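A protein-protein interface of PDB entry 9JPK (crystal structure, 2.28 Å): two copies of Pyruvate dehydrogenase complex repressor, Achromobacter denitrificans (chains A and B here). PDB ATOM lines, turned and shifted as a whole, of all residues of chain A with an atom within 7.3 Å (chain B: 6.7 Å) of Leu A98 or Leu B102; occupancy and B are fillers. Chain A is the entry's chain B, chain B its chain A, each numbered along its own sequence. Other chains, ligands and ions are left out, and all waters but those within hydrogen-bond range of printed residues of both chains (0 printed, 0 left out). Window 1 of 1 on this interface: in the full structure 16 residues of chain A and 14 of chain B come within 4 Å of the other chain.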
ATOM      1  N   LEU A  92      17.395  -6.122 -27.830  1.00  0.00           N
ATOM      2  CA  LEU A  92      17.480  -5.017 -26.865  1.00  0.00           C
ATOM      3  C   LEU A  92      17.029  -5.536 -25.518  1.00  0.00           C
ATOM      4  O   LEU A  92      17.681  -5.286 -24.540  1.00  0.00           O
ATOM      5  CB  LEU A  92      16.504  -3.943 -27.331  1.00  0.00           C
ATOM      6  CG  LEU A  92      16.682  -2.522 -26.822  1.00  0.00           C
ATOM      7  CD1 LEU A  92      18.130  -2.156 -26.759  1.00  0.00           C
ATOM      8  CD2 LEU A  92      15.962  -1.588 -27.753  1.00  0.00           C
ATOM      9  N   ALA A  93      15.964  -6.309 -25.523  1.00  0.00           N
ATOM     10  CA  ALA A  93      15.374  -6.776 -24.257  1.00  0.00           C
ATOM     11  C   ALA A  93      16.343  -7.653 -23.456  1.00  0.00           C
ATOM     12  O   ALA A  93      16.197  -7.659 -22.296  1.00  0.00           O
ATOM     13  CB  ALA A  93      14.032  -7.420 -24.476  1.00  0.00           C
ATOM     14  N   SER A  94      17.175  -8.412 -24.140  1.00  0.00           N
ATOM     15  CA  SER A  94      18.197  -9.308 -23.570  1.00  0.00           C
ATOM     16  C   SER A  94      19.252  -8.520 -22.789  1.00  0.00           C
ATOM     17  O   SER A  94      19.710  -9.014 -21.797  1.00  0.00           O
ATOM     18  CB  SER A  94      18.793 -10.134 -24.646  1.00  0.00           C
ATOM     19  OG  SER A  94      17.961 -11.223 -24.938  1.00  0.00           O
ATOM     20  N   VAL A  95      19.692  -7.386 -23.328  1.00  0.00           N
ATOM     21  CA  VAL A  95      20.624  -6.456 -22.641  1.00  0.00           C
ATOM     22  C   VAL A  95      19.882  -5.839 -21.457  1.00  0.00           C
ATOM     23  O   VAL A  95      20.430  -5.720 -20.422  1.00  0.00           O
ATOM     24  CB  VAL A  95      21.223  -5.401 -23.586  1.00  0.00           C
ATOM     25  CG1 VAL A  95      22.074  -4.437 -22.811  1.00  0.00           C
ATOM     26  CG2 VAL A  95      22.055  -6.059 -24.664  1.00  0.00           C
ATOM     27  N   TYR A  96      18.628  -5.489 -21.662  1.00  0.00           N
ATOM     28  CA  TYR A  96      17.890  -4.837 -20.565  1.00  0.00           C
ATOM     29  C   TYR A  96      17.761  -5.777 -19.373  1.00  0.00           C
ATOM     30  O   TYR A  96      17.836  -5.304 -18.287  1.00  0.00           O
ATOM     31  CB  TYR A  96      16.540  -4.316 -21.036  1.00  0.00           C
ATOM     32  CG  TYR A  96      16.466  -2.826 -21.237  1.00  0.00           C
ATOM     33  CD1 TYR A  96      16.349  -1.969 -20.168  1.00  0.00           C
ATOM     34  CD2 TYR A  96      16.478  -2.280 -22.497  1.00  0.00           C
ATOM     35  CE1 TYR A  96      16.245  -0.601 -20.348  1.00  0.00           C
ATOM     36  CE2 TYR A  96      16.400  -0.920 -22.698  1.00  0.00           C
ATOM     37  CZ  TYR A  96      16.285  -0.073 -21.622  1.00  0.00           C
ATOM     38  OH  TYR A  96      16.204   1.274 -21.833  1.00  0.00           O
ATOM     39  N   GLU A  97      17.515  -7.051 -19.625  1.00  0.00           N
ATOM     40  CA  GLU A  97      17.385  -8.089 -18.585  1.00  0.00           C
ATOM     41  C   GLU A  97      18.699  -8.208 -17.798  1.00  0.00           C
ATOM     42  O   GLU A  97      18.610  -8.124 -16.612  1.00  0.00           O
ATOM     43  CB  GLU A  97      16.991  -9.371 -19.318  1.00  0.00           C
ATOM     44  CG  GLU A  97      16.898 -10.651 -18.542  1.00  0.00           C
ATOM     45  CD  GLU A  97      16.152 -11.742 -19.313  1.00  0.00           C
ATOM     46  OE1 GLU A  97      14.992 -11.889 -19.085  1.00  0.00           O
ATOM     47  OE2 GLU A  97      16.708 -12.362 -20.152  1.00  0.00           O
ATOM     48  N   LEU A  98      19.838  -8.308 -18.480  1.00  0.00           N
ATOM     49  CA  LEU A  98      21.172  -8.425 -17.844  1.00  0.00           C
ATOM     50  C   LEU A  98      21.485  -7.169 -17.018  1.00  0.00           C
ATOM     51  O   LEU A  98      21.975  -7.310 -15.937  1.00  0.00           O
ATOM     52  CB  LEU A  98      22.235  -8.659 -18.912  1.00  0.00           C
ATOM     53  CG  LEU A  98      23.659  -8.838 -18.401  1.00  0.00           C
ATOM     54  CD1 LEU A  98      23.765 -10.094 -17.570  1.00  0.00           C
ATOM     55  CD2 LEU A  98      24.641  -8.887 -19.538  1.00  0.00           C
ATOM     56  N   ARG A  99      21.151  -5.991 -17.528  1.00  0.00           N
ATOM     57  CA  ARG A  99      21.403  -4.730 -16.803  1.00  0.00           C
ATOM     58  C   ARG A  99      20.570  -4.708 -15.533  1.00  0.00           C
ATOM     59  O   ARG A  99      21.067  -4.300 -14.527  1.00  0.00           O
ATOM     60  CB  ARG A  99      21.100  -3.507 -17.663  1.00  0.00           C
ATOM     61  CG  ARG A  99      21.645  -2.221 -17.073  1.00  0.00           C
ATOM     62  CD  ARG A  99      20.643  -1.227 -16.549  1.00  0.00           C
ATOM     63  NE  ARG A  99      20.242  -0.412 -17.665  1.00  0.00           N
ATOM     64  CZ  ARG A  99      19.009  -0.226 -18.073  1.00  0.00           C
ATOM     65  NH1 ARG A  99      17.991  -0.752 -17.424  1.00  0.00           N
ATOM     66  NH2 ARG A  99      18.784   0.510 -19.129  1.00  0.00           N
ATOM     67  N   MET A 100      19.345  -5.190 -15.630  1.00  0.00           N
ATOM     68  CA  MET A 100      18.420  -5.218 -14.482  1.00  0.00           C
ATOM     69  C   MET A 100      19.035  -6.046 -13.361  1.00  0.00           C
ATOM     70  O   MET A 100      18.995  -5.582 -12.260  1.00  0.00           O
ATOM     71  CB  MET A 100      17.087  -5.847 -14.883  1.00  0.00           C
ATOM     72  CG  MET A 100      16.150  -6.005 -13.726  1.00  0.00           C
ATOM     73  SD  MET A 100      14.468  -6.268 -14.209  1.00  0.00           S
ATOM     74  CE  MET A 100      14.356  -5.252 -15.673  1.00  0.00           C
ATOM     75  N   GLU A 101      19.600  -7.203 -13.670  1.00  0.00           N
ATOM     76  CA  GLU A 101      20.207  -8.086 -12.647  1.00  0.00           C
ATOM     77  C   GLU A 101      21.405  -7.416 -11.984  1.00  0.00           C
ATOM     78  O   GLU A 101      21.458  -7.427 -10.783  1.00  0.00           O
ATOM     79  CB  GLU A 101      20.669  -9.384 -13.293  1.00  0.00           C
ATOM     80  CG  GLU A 101      19.553 -10.371 -13.474  1.00  0.00           C
ATOM     81  CD  GLU A 101      18.867 -10.641 -12.157  1.00  0.00           C
ATOM     82  OE1 GLU A 101      19.562 -10.777 -11.165  1.00  0.00           O
ATOM     83  OE2 GLU A 101      17.669 -10.633 -12.124  1.00  0.00           O
ATOM     84  N   LEU A 102      22.291  -6.837 -12.784  1.00  0.00           N
ATOM     85  CA  LEU A 102      23.518  -6.147 -12.323  1.00  0.00           C
ATOM     86  C   LEU A 102      23.195  -4.881 -11.539  1.00  0.00           C
ATOM     87  O   LEU A 102      23.792  -4.715 -10.523  1.00  0.00           O
ATOM     88  CB  LEU A 102      24.325  -5.756 -13.551  1.00  0.00           C
ATOM     89  CG  LEU A 102      25.216  -6.842 -14.092  1.00  0.00           C
ATOM     90  CD1 LEU A 102      26.017  -6.313 -15.254  1.00  0.00           C
ATOM     91  CD2 LEU A 102      26.067  -7.366 -12.954  1.00  0.00           C
ATOM     92  N   GLU A 103      22.243  -4.068 -11.995  1.00  0.00           N
ATOM     93  CA  GLU A 103      21.880  -2.822 -11.269  1.00  0.00           C
ATOM     94  C   GLU A 103      21.338  -3.167  -9.885  1.00  0.00           C
ATOM     95  O   GLU A 103      21.678  -2.481  -8.956  1.00  0.00           O
ATOM     96  CB  GLU A 103      20.889  -1.953 -12.039  1.00  0.00           C
ATOM     97  CG  GLU A 103      21.530  -1.151 -13.148  1.00  0.00           C
ATOM     98  CD  GLU A 103      21.642   0.358 -13.038  1.00  0.00           C
ATOM     99  OE1 GLU A 103      21.471   0.899 -11.942  1.00  0.00           O
ATOM    100  OE2 GLU A 103      21.890   0.973 -14.066  1.00  0.00           O
ATOM    101  N   GLY A 104      20.558  -4.235  -9.780  1.00  0.00           N
ATOM    102  CA  GLY A 104      20.021  -4.680  -8.488  1.00  0.00           C
ATOM    103  C   GLY A 104      21.154  -5.014  -7.552  1.00  0.00           C
ATOM    104  O   GLY A 104      21.104  -4.580  -6.436  1.00  0.00           O
ATOM    105  N   TYR A 159      32.993  -4.706 -11.861  1.00  0.00           N
ATOM    106  CA  TYR A 159      31.530  -4.518 -11.829  1.00  0.00           C
ATOM    107  C   TYR A 159      31.138  -3.199 -12.498  1.00  0.00           C
ATOM    108  O   TYR A 159      30.198  -3.193 -13.197  1.00  0.00           O
ATOM    109  CB  TYR A 159      31.063  -4.501 -10.374  1.00  0.00           C
ATOM    110  CG  TYR A 159      29.669  -4.996 -10.094  1.00  0.00           C
ATOM    111  CD1 TYR A 159      28.557  -4.397 -10.641  1.00  0.00           C
ATOM    112  CD2 TYR A 159      29.473  -6.069  -9.256  1.00  0.00           C
ATOM    113  CE1 TYR A 159      27.295  -4.882 -10.398  1.00  0.00           C
ATOM    114  CE2 TYR A 159      28.217  -6.545  -8.970  1.00  0.00           C
ATOM    115  CZ  TYR A 159      27.124  -5.952  -9.549  1.00  0.00           C
ATOM    116  OH  TYR A 159      25.907  -6.440  -9.307  1.00  0.00           O
ATOM    117  N   LEU A 162      31.656  -3.251 -16.413  1.00  0.00           N
ATOM    118  CA  LEU A 162      30.576  -3.972 -17.112  1.00  0.00           C
ATOM    119  C   LEU A 162      29.258  -3.193 -17.130  1.00  0.00           C
ATOM    120  O   LEU A 162      28.633  -3.143 -18.151  1.00  0.00           O
ATOM    121  CB  LEU A 162      30.370  -5.361 -16.545  1.00  0.00           C
ATOM    122  CG  LEU A 162      29.386  -6.164 -17.368  1.00  0.00           C
ATOM    123  CD1 LEU A 162      29.841  -6.206 -18.802  1.00  0.00           C
ATOM    124  CD2 LEU A 162      29.241  -7.549 -16.815  1.00  0.00           C
ATOM    125  N   LEU A 163      28.892  -2.588 -16.016  1.00  0.00           N
ATOM    126  CA  LEU A 163      27.667  -1.783 -15.944  1.00  0.00           C
ATOM    127  C   LEU A 163      27.797  -0.592 -16.885  1.00  0.00           C
ATOM    128  O   LEU A 163      26.833  -0.272 -17.510  1.00  0.00           O
ATOM    129  CB  LEU A 163      27.417  -1.363 -14.505  1.00  0.00           C
ATOM    130  CG  LEU A 163      26.266  -2.059 -13.803  1.00  0.00           C
ATOM    131  CD1 LEU A 163      26.039  -1.544 -12.409  1.00  0.00           C
ATOM    132  CD2 LEU A 163      24.988  -1.974 -14.608  1.00  0.00           C
ATOM    133  N   LEU A 166      27.317  -1.873 -20.569  1.00  0.00           N
ATOM    134  CA  LEU A 166      25.907  -2.222 -20.853  1.00  0.00           C
ATOM    135  C   LEU A 166      25.062  -0.942 -20.968  1.00  0.00           C
ATOM    136  O   LEU A 166      24.252  -0.875 -21.822  1.00  0.00           O
ATOM    137  CB  LEU A 166      25.337  -3.170 -19.802  1.00  0.00           C
ATOM    138  CG  LEU A 166      26.017  -4.515 -19.616  1.00  0.00           C
ATOM    139  CD1 LEU A 166      25.369  -5.273 -18.497  1.00  0.00           C
ATOM    140  CD2 LEU A 166      25.972  -5.349 -20.872  1.00  0.00           C
ATOM    141  N   LEU A 218      13.944  -0.366 -12.515  1.00  0.00           N
ATOM    142  CA  LEU A 218      14.220  -0.908 -13.856  1.00  0.00           C
ATOM    143  C   LEU A 218      12.978  -1.595 -14.438  1.00  0.00           C
ATOM    144  O   LEU A 218      12.825  -1.574 -15.605  1.00  0.00           O
ATOM    145  CB  LEU A 218      15.517  -1.718 -13.868  1.00  0.00           C
ATOM    146  CG  LEU A 218      16.797  -0.995 -13.447  1.00  0.00           C
ATOM    147  CD1 LEU A 218      18.012  -1.751 -13.890  1.00  0.00           C
ATOM    148  CD2 LEU A 218      16.879   0.403 -13.975  1.00  0.00           C
ATOM    149  N   GLU B  97      33.027 -11.544  -6.933  1.00  0.00           N
ATOM    150  CA  GLU B  97      31.858 -10.728  -6.501  1.00  0.00           C
ATOM    151  C   GLU B  97      30.931 -10.452  -7.702  1.00  0.00           C
ATOM    152  O   GLU B  97      29.780 -10.653  -7.572  1.00  0.00           O
ATOM    153  CB  GLU B  97      32.381  -9.519  -5.739  1.00  0.00           C
ATOM    154  CG  GLU B  97      31.365  -8.474  -5.409  1.00  0.00           C
ATOM    155  CD  GLU B  97      31.812  -7.335  -4.483  1.00  0.00           C
ATOM    156  OE1 GLU B  97      32.355  -6.330  -4.956  1.00  0.00           O
ATOM    157  OE2 GLU B  97      31.615  -7.489  -3.293  1.00  0.00           O
ATOM    158  N   LEU B  98      31.495 -10.076  -8.838  1.00  0.00           N
ATOM    159  CA  LEU B  98      30.767  -9.854 -10.106  1.00  0.00           C
ATOM    160  C   LEU B  98      30.211 -11.176 -10.632  1.00  0.00           C
ATOM    161  O   LEU B  98      29.083 -11.200 -11.035  1.00  0.00           O
ATOM    162  CB  LEU B  98      31.696  -9.221 -11.132  1.00  0.00           C
ATOM    163  CG  LEU B  98      31.099  -9.131 -12.522  1.00  0.00           C
ATOM    164  CD1 LEU B  98      29.744  -8.515 -12.474  1.00  0.00           C
ATOM    165  CD2 LEU B  98      31.988  -8.401 -13.492  1.00  0.00           C
ATOM    166  N   ARG B  99      31.005 -12.232 -10.543  1.00  0.00           N
ATOM    167  CA  ARG B  99      30.609 -13.581 -10.974  1.00  0.00           C
ATOM    168  C   ARG B  99      29.461 -14.037 -10.093  1.00  0.00           C
ATOM    169  O   ARG B  99      28.543 -14.560 -10.648  1.00  0.00           O
ATOM    170  CB  ARG B  99      31.799 -14.538 -11.059  1.00  0.00           C
ATOM    171  CG  ARG B  99      31.493 -15.929 -11.598  1.00  0.00           C
ATOM    172  CD  ARG B  99      31.273 -16.145 -13.081  1.00  0.00           C
ATOM    173  NE  ARG B  99      30.881 -17.512 -13.337  1.00  0.00           N
ATOM    174  CZ  ARG B  99      31.674 -18.557 -13.528  1.00  0.00           C
ATOM    175  NH1 ARG B  99      32.975 -18.423 -13.539  1.00  0.00           N
ATOM    176  NH2 ARG B  99      31.141 -19.752 -13.698  1.00  0.00           N
ATOM    177  N   MET B 100      29.492 -13.722  -8.803  1.00  0.00           N
ATOM    178  CA  MET B 100      28.453 -14.161  -7.869  1.00  0.00           C
ATOM    179  C   MET B 100      27.095 -13.620  -8.275  1.00  0.00           C
ATOM    180  O   MET B 100      26.210 -14.396  -8.384  1.00  0.00           O
ATOM    181  CB  MET B 100      28.816 -13.695  -6.471  1.00  0.00           C
ATOM    182  CG  MET B 100      27.811 -13.932  -5.421  1.00  0.00           C
ATOM    183  SD  MET B 100      28.581 -13.632  -3.843  1.00  0.00           S
ATOM    184  CE  MET B 100      27.999 -11.992  -3.490  1.00  0.00           C
ATOM    185  N   GLU B 101      27.020 -12.335  -8.569  1.00  0.00           N
ATOM    186  CA  GLU B 101      25.788 -11.652  -8.999  1.00  0.00           C
ATOM    187  C   GLU B 101      25.295 -12.199 -10.327  1.00  0.00           C
ATOM    188  O   GLU B 101      24.146 -12.405 -10.400  1.00  0.00           O
ATOM    189  CB  GLU B 101      26.068 -10.163  -9.172  1.00  0.00           C
ATOM    190  CG  GLU B 101      24.856  -9.316  -9.045  1.00  0.00           C
ATOM    191  CD  GLU B 101      23.966  -9.613  -7.856  1.00  0.00           C
ATOM    192  OE1 GLU B 101      22.739  -9.658  -8.049  1.00  0.00           O
ATOM    193  OE2 GLU B 101      24.488  -9.779  -6.777  1.00  0.00           O
ATOM    194  N   LEU B 102      26.172 -12.407 -11.305  1.00  0.00           N
ATOM    195  CA  LEU B 102      25.784 -12.945 -12.639  1.00  0.00           C
ATOM    196  C   LEU B 102      25.226 -14.379 -12.560  1.00  0.00           C
ATOM    197  O   LEU B 102      24.248 -14.627 -13.192  1.00  0.00           O
ATOM    198  CB  LEU B 102      26.940 -12.814 -13.635  1.00  0.00           C
ATOM    199  CG  LEU B 102      27.225 -11.410 -14.170  1.00  0.00           C
ATOM    200  CD1 LEU B 102      28.572 -11.339 -14.801  1.00  0.00           C
ATOM    201  CD2 LEU B 102      26.172 -10.907 -15.130  1.00  0.00           C
ATOM    202  N   GLU B 103      25.830 -15.240 -11.740  1.00  0.00           N
ATOM    203  CA  GLU B 103      25.420 -16.652 -11.501  1.00  0.00           C
ATOM    204  C   GLU B 103      24.038 -16.723 -10.851  1.00  0.00           C
ATOM    205  O   GLU B 103      23.294 -17.546 -11.244  1.00  0.00           O
ATOM    206  CB  GLU B 103      26.468 -17.419 -10.698  1.00  0.00           C
ATOM    207  CG  GLU B 103      27.739 -17.697 -11.441  1.00  0.00           C
ATOM    208  CD  GLU B 103      27.806 -18.906 -12.348  1.00  0.00           C
ATOM    209  OE1 GLU B 103      28.675 -18.929 -13.165  1.00  0.00           O
ATOM    210  OE2 GLU B 103      27.014 -19.802 -12.205  1.00  0.00           O
ATOM    211  N   GLY B 104      23.761 -15.834  -9.902  1.00  0.00           N
ATOM    212  CA  GLY B 104      22.457 -15.709  -9.235  1.00  0.00           C
ATOM    213  C   GLY B 104      21.345 -15.336 -10.202  1.00  0.00           C
ATOM    214  O   GLY B 104      20.279 -15.882 -10.098  1.00  0.00           O
ATOM    215  N   GLY B 105      21.619 -14.384 -11.092  1.00  0.00           N
ATOM    216  CA  GLY B 105      20.674 -13.990 -12.145  1.00  0.00           C
ATOM    217  C   GLY B 105      20.457 -15.122 -13.125  1.00  0.00           C
ATOM    218  O   GLY B 105      19.376 -15.333 -13.496  1.00  0.00           O
ATOM    219  N   ALA B 106      21.520 -15.808 -13.498  1.00  0.00           N
ATOM    220  CA  ALA B 106      21.438 -16.945 -14.429  1.00  0.00           C
ATOM    221  C   ALA B 106      20.645 -18.078 -13.788  1.00  0.00           C
ATOM    222  O   ALA B 106      19.828 -18.568 -14.436  1.00  0.00           O
ATOM    223  CB  ALA B 106      22.790 -17.392 -14.888  1.00  0.00           C
ATOM    224  N   ALA B 107      20.852 -18.379 -12.518  1.00  0.00           N
ATOM    225  CA  ALA B 107      20.098 -19.484 -11.902  1.00  0.00           C
ATOM    226  C   ALA B 107      18.601 -19.190 -11.829  1.00  0.00           C
ATOM    227  O   ALA B 107      17.856 -20.104 -11.951  1.00  0.00           O
ATOM    228  CB  ALA B 107      20.680 -19.907 -10.592  1.00  0.00           C
ATOM    229  N   LEU B 109      16.921 -17.090 -13.841  1.00  0.00           N
ATOM    230  CA  LEU B 109      16.361 -17.142 -15.200  1.00  0.00           C
ATOM    231  C   LEU B 109      16.209 -18.603 -15.614  1.00  0.00           C
ATOM    232  O   LEU B 109      15.165 -18.941 -16.101  1.00  0.00           O
ATOM    233  CB  LEU B 109      17.233 -16.350 -16.177  1.00  0.00           C
ATOM    234  CG  LEU B 109      17.282 -14.841 -15.958  1.00  0.00           C
ATOM    235  CD1 LEU B 109      18.020 -14.176 -17.078  1.00  0.00           C
ATOM    236  CD2 LEU B 109      15.901 -14.243 -15.870  1.00  0.00           C
ATOM    237  N   ASN B 156      18.955 -16.320 -22.896  1.00  0.00           N
ATOM    238  CA  ASN B 156      19.311 -14.918 -23.137  1.00  0.00           C
ATOM    239  C   ASN B 156      20.660 -15.085 -23.749  1.00  0.00           C
ATOM    240  O   ASN B 156      21.535 -15.478 -23.036  1.00  0.00           O
ATOM    241  CB  ASN B 156      19.484 -14.158 -21.825  1.00  0.00           C
ATOM    242  CG  ASN B 156      19.846 -12.704 -22.010  1.00  0.00           C
ATOM    243  OD1 ASN B 156      20.698 -12.380 -22.787  1.00  0.00           O
ATOM    244  ND2 ASN B 156      19.181 -11.842 -21.297  1.00  0.00           N
ATOM    245  N   TYR B 158      22.794 -12.876 -24.711  1.00  0.00           N
ATOM    246  CA  TYR B 158      23.820 -11.969 -24.163  1.00  0.00           C
ATOM    247  C   TYR B 158      24.435 -12.516 -22.879  1.00  0.00           C
ATOM    248  O   TYR B 158      25.617 -12.687 -22.821  1.00  0.00           O
ATOM    249  CB  TYR B 158      23.249 -10.558 -24.059  1.00  0.00           C
ATOM    250  CG  TYR B 158      24.316  -9.544 -24.266  1.00  0.00           C
ATOM    251  CD1 TYR B 158      24.707  -9.131 -25.515  1.00  0.00           C
ATOM    252  CD2 TYR B 158      24.999  -9.062 -23.182  1.00  0.00           C
ATOM    253  CE1 TYR B 158      25.743  -8.222 -25.662  1.00  0.00           C
ATOM    254  CE2 TYR B 158      26.013  -8.140 -23.301  1.00  0.00           C
ATOM    255  CZ  TYR B 158      26.391  -7.717 -24.545  1.00  0.00           C
ATOM    256  OH  TYR B 158      27.442  -6.862 -24.594  1.00  0.00           O
ATOM    257  N   TYR B 159      23.583 -12.944 -21.973  1.00  0.00           N
ATOM    258  CA  TYR B 159      23.971 -13.518 -20.672  1.00  0.00           C
ATOM    259  C   TYR B 159      24.771 -14.804 -20.898  1.00  0.00           C
ATOM    260  O   TYR B 159      25.749 -15.044 -20.278  1.00  0.00           O
ATOM    261  CB  TYR B 159      22.658 -13.773 -19.948  1.00  0.00           C
ATOM    262  CG  TYR B 159      22.591 -13.462 -18.490  1.00  0.00           C
ATOM    263  CD1 TYR B 159      23.591 -13.868 -17.657  1.00  0.00           C
ATOM    264  CD2 TYR B 159      21.504 -12.832 -17.949  1.00  0.00           C
ATOM    265  CE1 TYR B 159      23.528 -13.633 -16.311  1.00  0.00           C
ATOM    266  CE2 TYR B 159      21.424 -12.574 -16.602  1.00  0.00           C
ATOM    267  CZ  TYR B 159      22.447 -12.991 -15.789  1.00  0.00           C
ATOM    268  OH  TYR B 159      22.439 -12.779 -14.468  1.00  0.00           O
ATOM    269  N   LEU B 162      28.369 -13.948 -22.338  1.00  0.00           N
ATOM    270  CA  LEU B 162      29.243 -13.353 -21.313  1.00  0.00           C
ATOM    271  C   LEU B 162      29.729 -14.463 -20.359  1.00  0.00           C
ATOM    272  O   LEU B 162      30.888 -14.467 -20.051  1.00  0.00           O
ATOM    273  CB  LEU B 162      28.426 -12.279 -20.592  1.00  0.00           C
ATOM    274  CG  LEU B 162      29.039 -11.714 -19.323  1.00  0.00           C
ATOM    275  CD1 LEU B 162      30.430 -11.202 -19.581  1.00  0.00           C
ATOM    276  CD2 LEU B 162      28.170 -10.647 -18.693  1.00  0.00           C
ATOM    277  N   LEU B 163      28.835 -15.370 -19.945  1.00  0.00           N
ATOM    278  CA  LEU B 163      29.131 -16.479 -18.982  1.00  0.00           C
ATOM    279  C   LEU B 163      30.061 -17.535 -19.567  1.00  0.00           C
ATOM    280  O   LEU B 163      30.968 -17.892 -18.897  1.00  0.00           O
ATOM    281  CB  LEU B 163      27.884 -17.033 -18.290  1.00  0.00           C
ATOM    282  CG  LEU B 163      27.349 -16.096 -17.212  1.00  0.00           C
ATOM    283  CD1 LEU B 163      25.954 -16.421 -16.782  1.00  0.00           C
ATOM    284  CD2 LEU B 163      28.266 -16.034 -16.024  1.00  0.00           C
ATOM    285  N   LEU B 166      33.391 -15.941 -19.288  1.00  0.00           N
ATOM    286  CA  LEU B 166      33.846 -15.853 -17.875  1.00  0.00           C
ATOM    287  C   LEU B 166      34.123 -17.227 -17.251  1.00  0.00           C
ATOM    288  O   LEU B 166      34.955 -17.281 -16.392  1.00  0.00           O
ATOM    289  CB  LEU B 166      32.893 -15.037 -17.012  1.00  0.00           C
ATOM    290  CG  LEU B 166      32.881 -13.555 -17.303  1.00  0.00           C
ATOM    291  CD1 LEU B 166      32.086 -12.810 -16.262  1.00  0.00           C
ATOM    292  CD2 LEU B 166      34.288 -13.052 -17.373  1.00  0.00           C
ATOM    293  N   THR B 215      24.507 -18.224  -5.641  1.00  0.00           N
ATOM    294  CA  THR B 215      25.269 -17.174  -4.938  1.00  0.00           C
ATOM    295  C   THR B 215      26.109 -17.793  -3.834  1.00  0.00           C
ATOM    296  O   THR B 215      27.196 -17.362  -3.658  1.00  0.00           O
ATOM    297  CB  THR B 215      24.449 -15.923  -4.612  1.00  0.00           C
ATOM    298  OG1 THR B 215      23.464 -16.136  -3.629  1.00  0.00           O
ATOM    299  CG2 THR B 215      23.768 -15.354  -5.821  1.00  0.00           C
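Leu A98 touches Tyr B159, but with the chains exchanged Tyr A159 does not touch Leu B98 (4.1 Å). Glu B101 touches its own counterpart, Glu A101. Glu A101 touches Tyr B159, and with the chains exchanged Tyr A159 touches Glu B101. Leu B162 touches its own counterpart, Leu A162.
Of the 19 printed residues of chain B, 9 touch a printed residue of chain A. Hydrophobic or aromatic side chains of chain B that line the printed part of chain A: Leu B98, Leu B102, Leu B109, Tyr B158, Tyr B159 and Leu B162. Of the 18 printed residues of chain A, 8 touch a printed residue of chain B. Among the printed residues, 13 pairs touch across the chains. Among the printed residues, no Asp or Glu carboxylate lies within 4 Å of a Lys or Arg side-chain nitrogen of the other chain.
Among the printed residues, pairs that only touch across the chains: Glu A97 with Leu B109, Leu A98 with Leu B102, Leu A98 with Tyr B158, Leu A98 with Tyr B159, Glu A101 with Glu B101, Glu A101 with Gly B105, Glu A101 with Tyr B159, Leu A102 with Leu B98, Tyr A159 with Glu B101, Leu A162 with Leu B162 and Leu A166 with Tyr B158.
O of Ser A94 lies within hydrogen-bond range of ND2 of Asn B156, at 2.9 Å. The side-chain amide nitrogen (ND2) of Asn B156 lies within hydrogen-bond range of the side-chain carboxylate (OE2) of Glu A97, 2.8 Å away.
Of chain B, only Leu B102 (3.5 Å), Tyr B158 (3.7 Å) and Tyr B159 (3.5 Å) come within 4 Å of Leu A98. Printed residues of chain B within 4 Å of Leu A102: Leu B98. Printed residues of chain B within 4 Å of Tyr A159: Glu B101 (3.1 Å). Of the printed residues of chain A, Gly B105 touches Glu A101 (3.5 Å). Of the printed residues of chain A, Asn B156 touches Ser A94 and Glu A97. Printed residues of chain A within 4 Å of Tyr B158: Leu A98 and Leu A166. The nearest residue of chain A that does not touch Leu B102 is Leu A102 (4.2 Å).
The backbone carbonyl oxygen (O) of Leu B102 is in hydrogen-bond range of the side-chain hydroxyl (OH) of Tyr B159. OH of Tyr B159 sits at hydrogen-bond distance from N of Ala B106, 3.3 Å away. The side-chain amide oxygen (OD1) of Asn B156 sits at hydrogen-bond distance from the backbone NH (N) of Tyr B158, at 2.9 Å. The side-chain amide oxygen (OD1) of Asn B156 lies within hydrogen-bond range of the backbone NH (N) of Tyr B159 (3.1 Å). The side-chain hydroxyl of Tyr A159 lies within hydrogen-bond range of the backbone carbonyl oxygen of Leu A102, 3.0 Å away.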
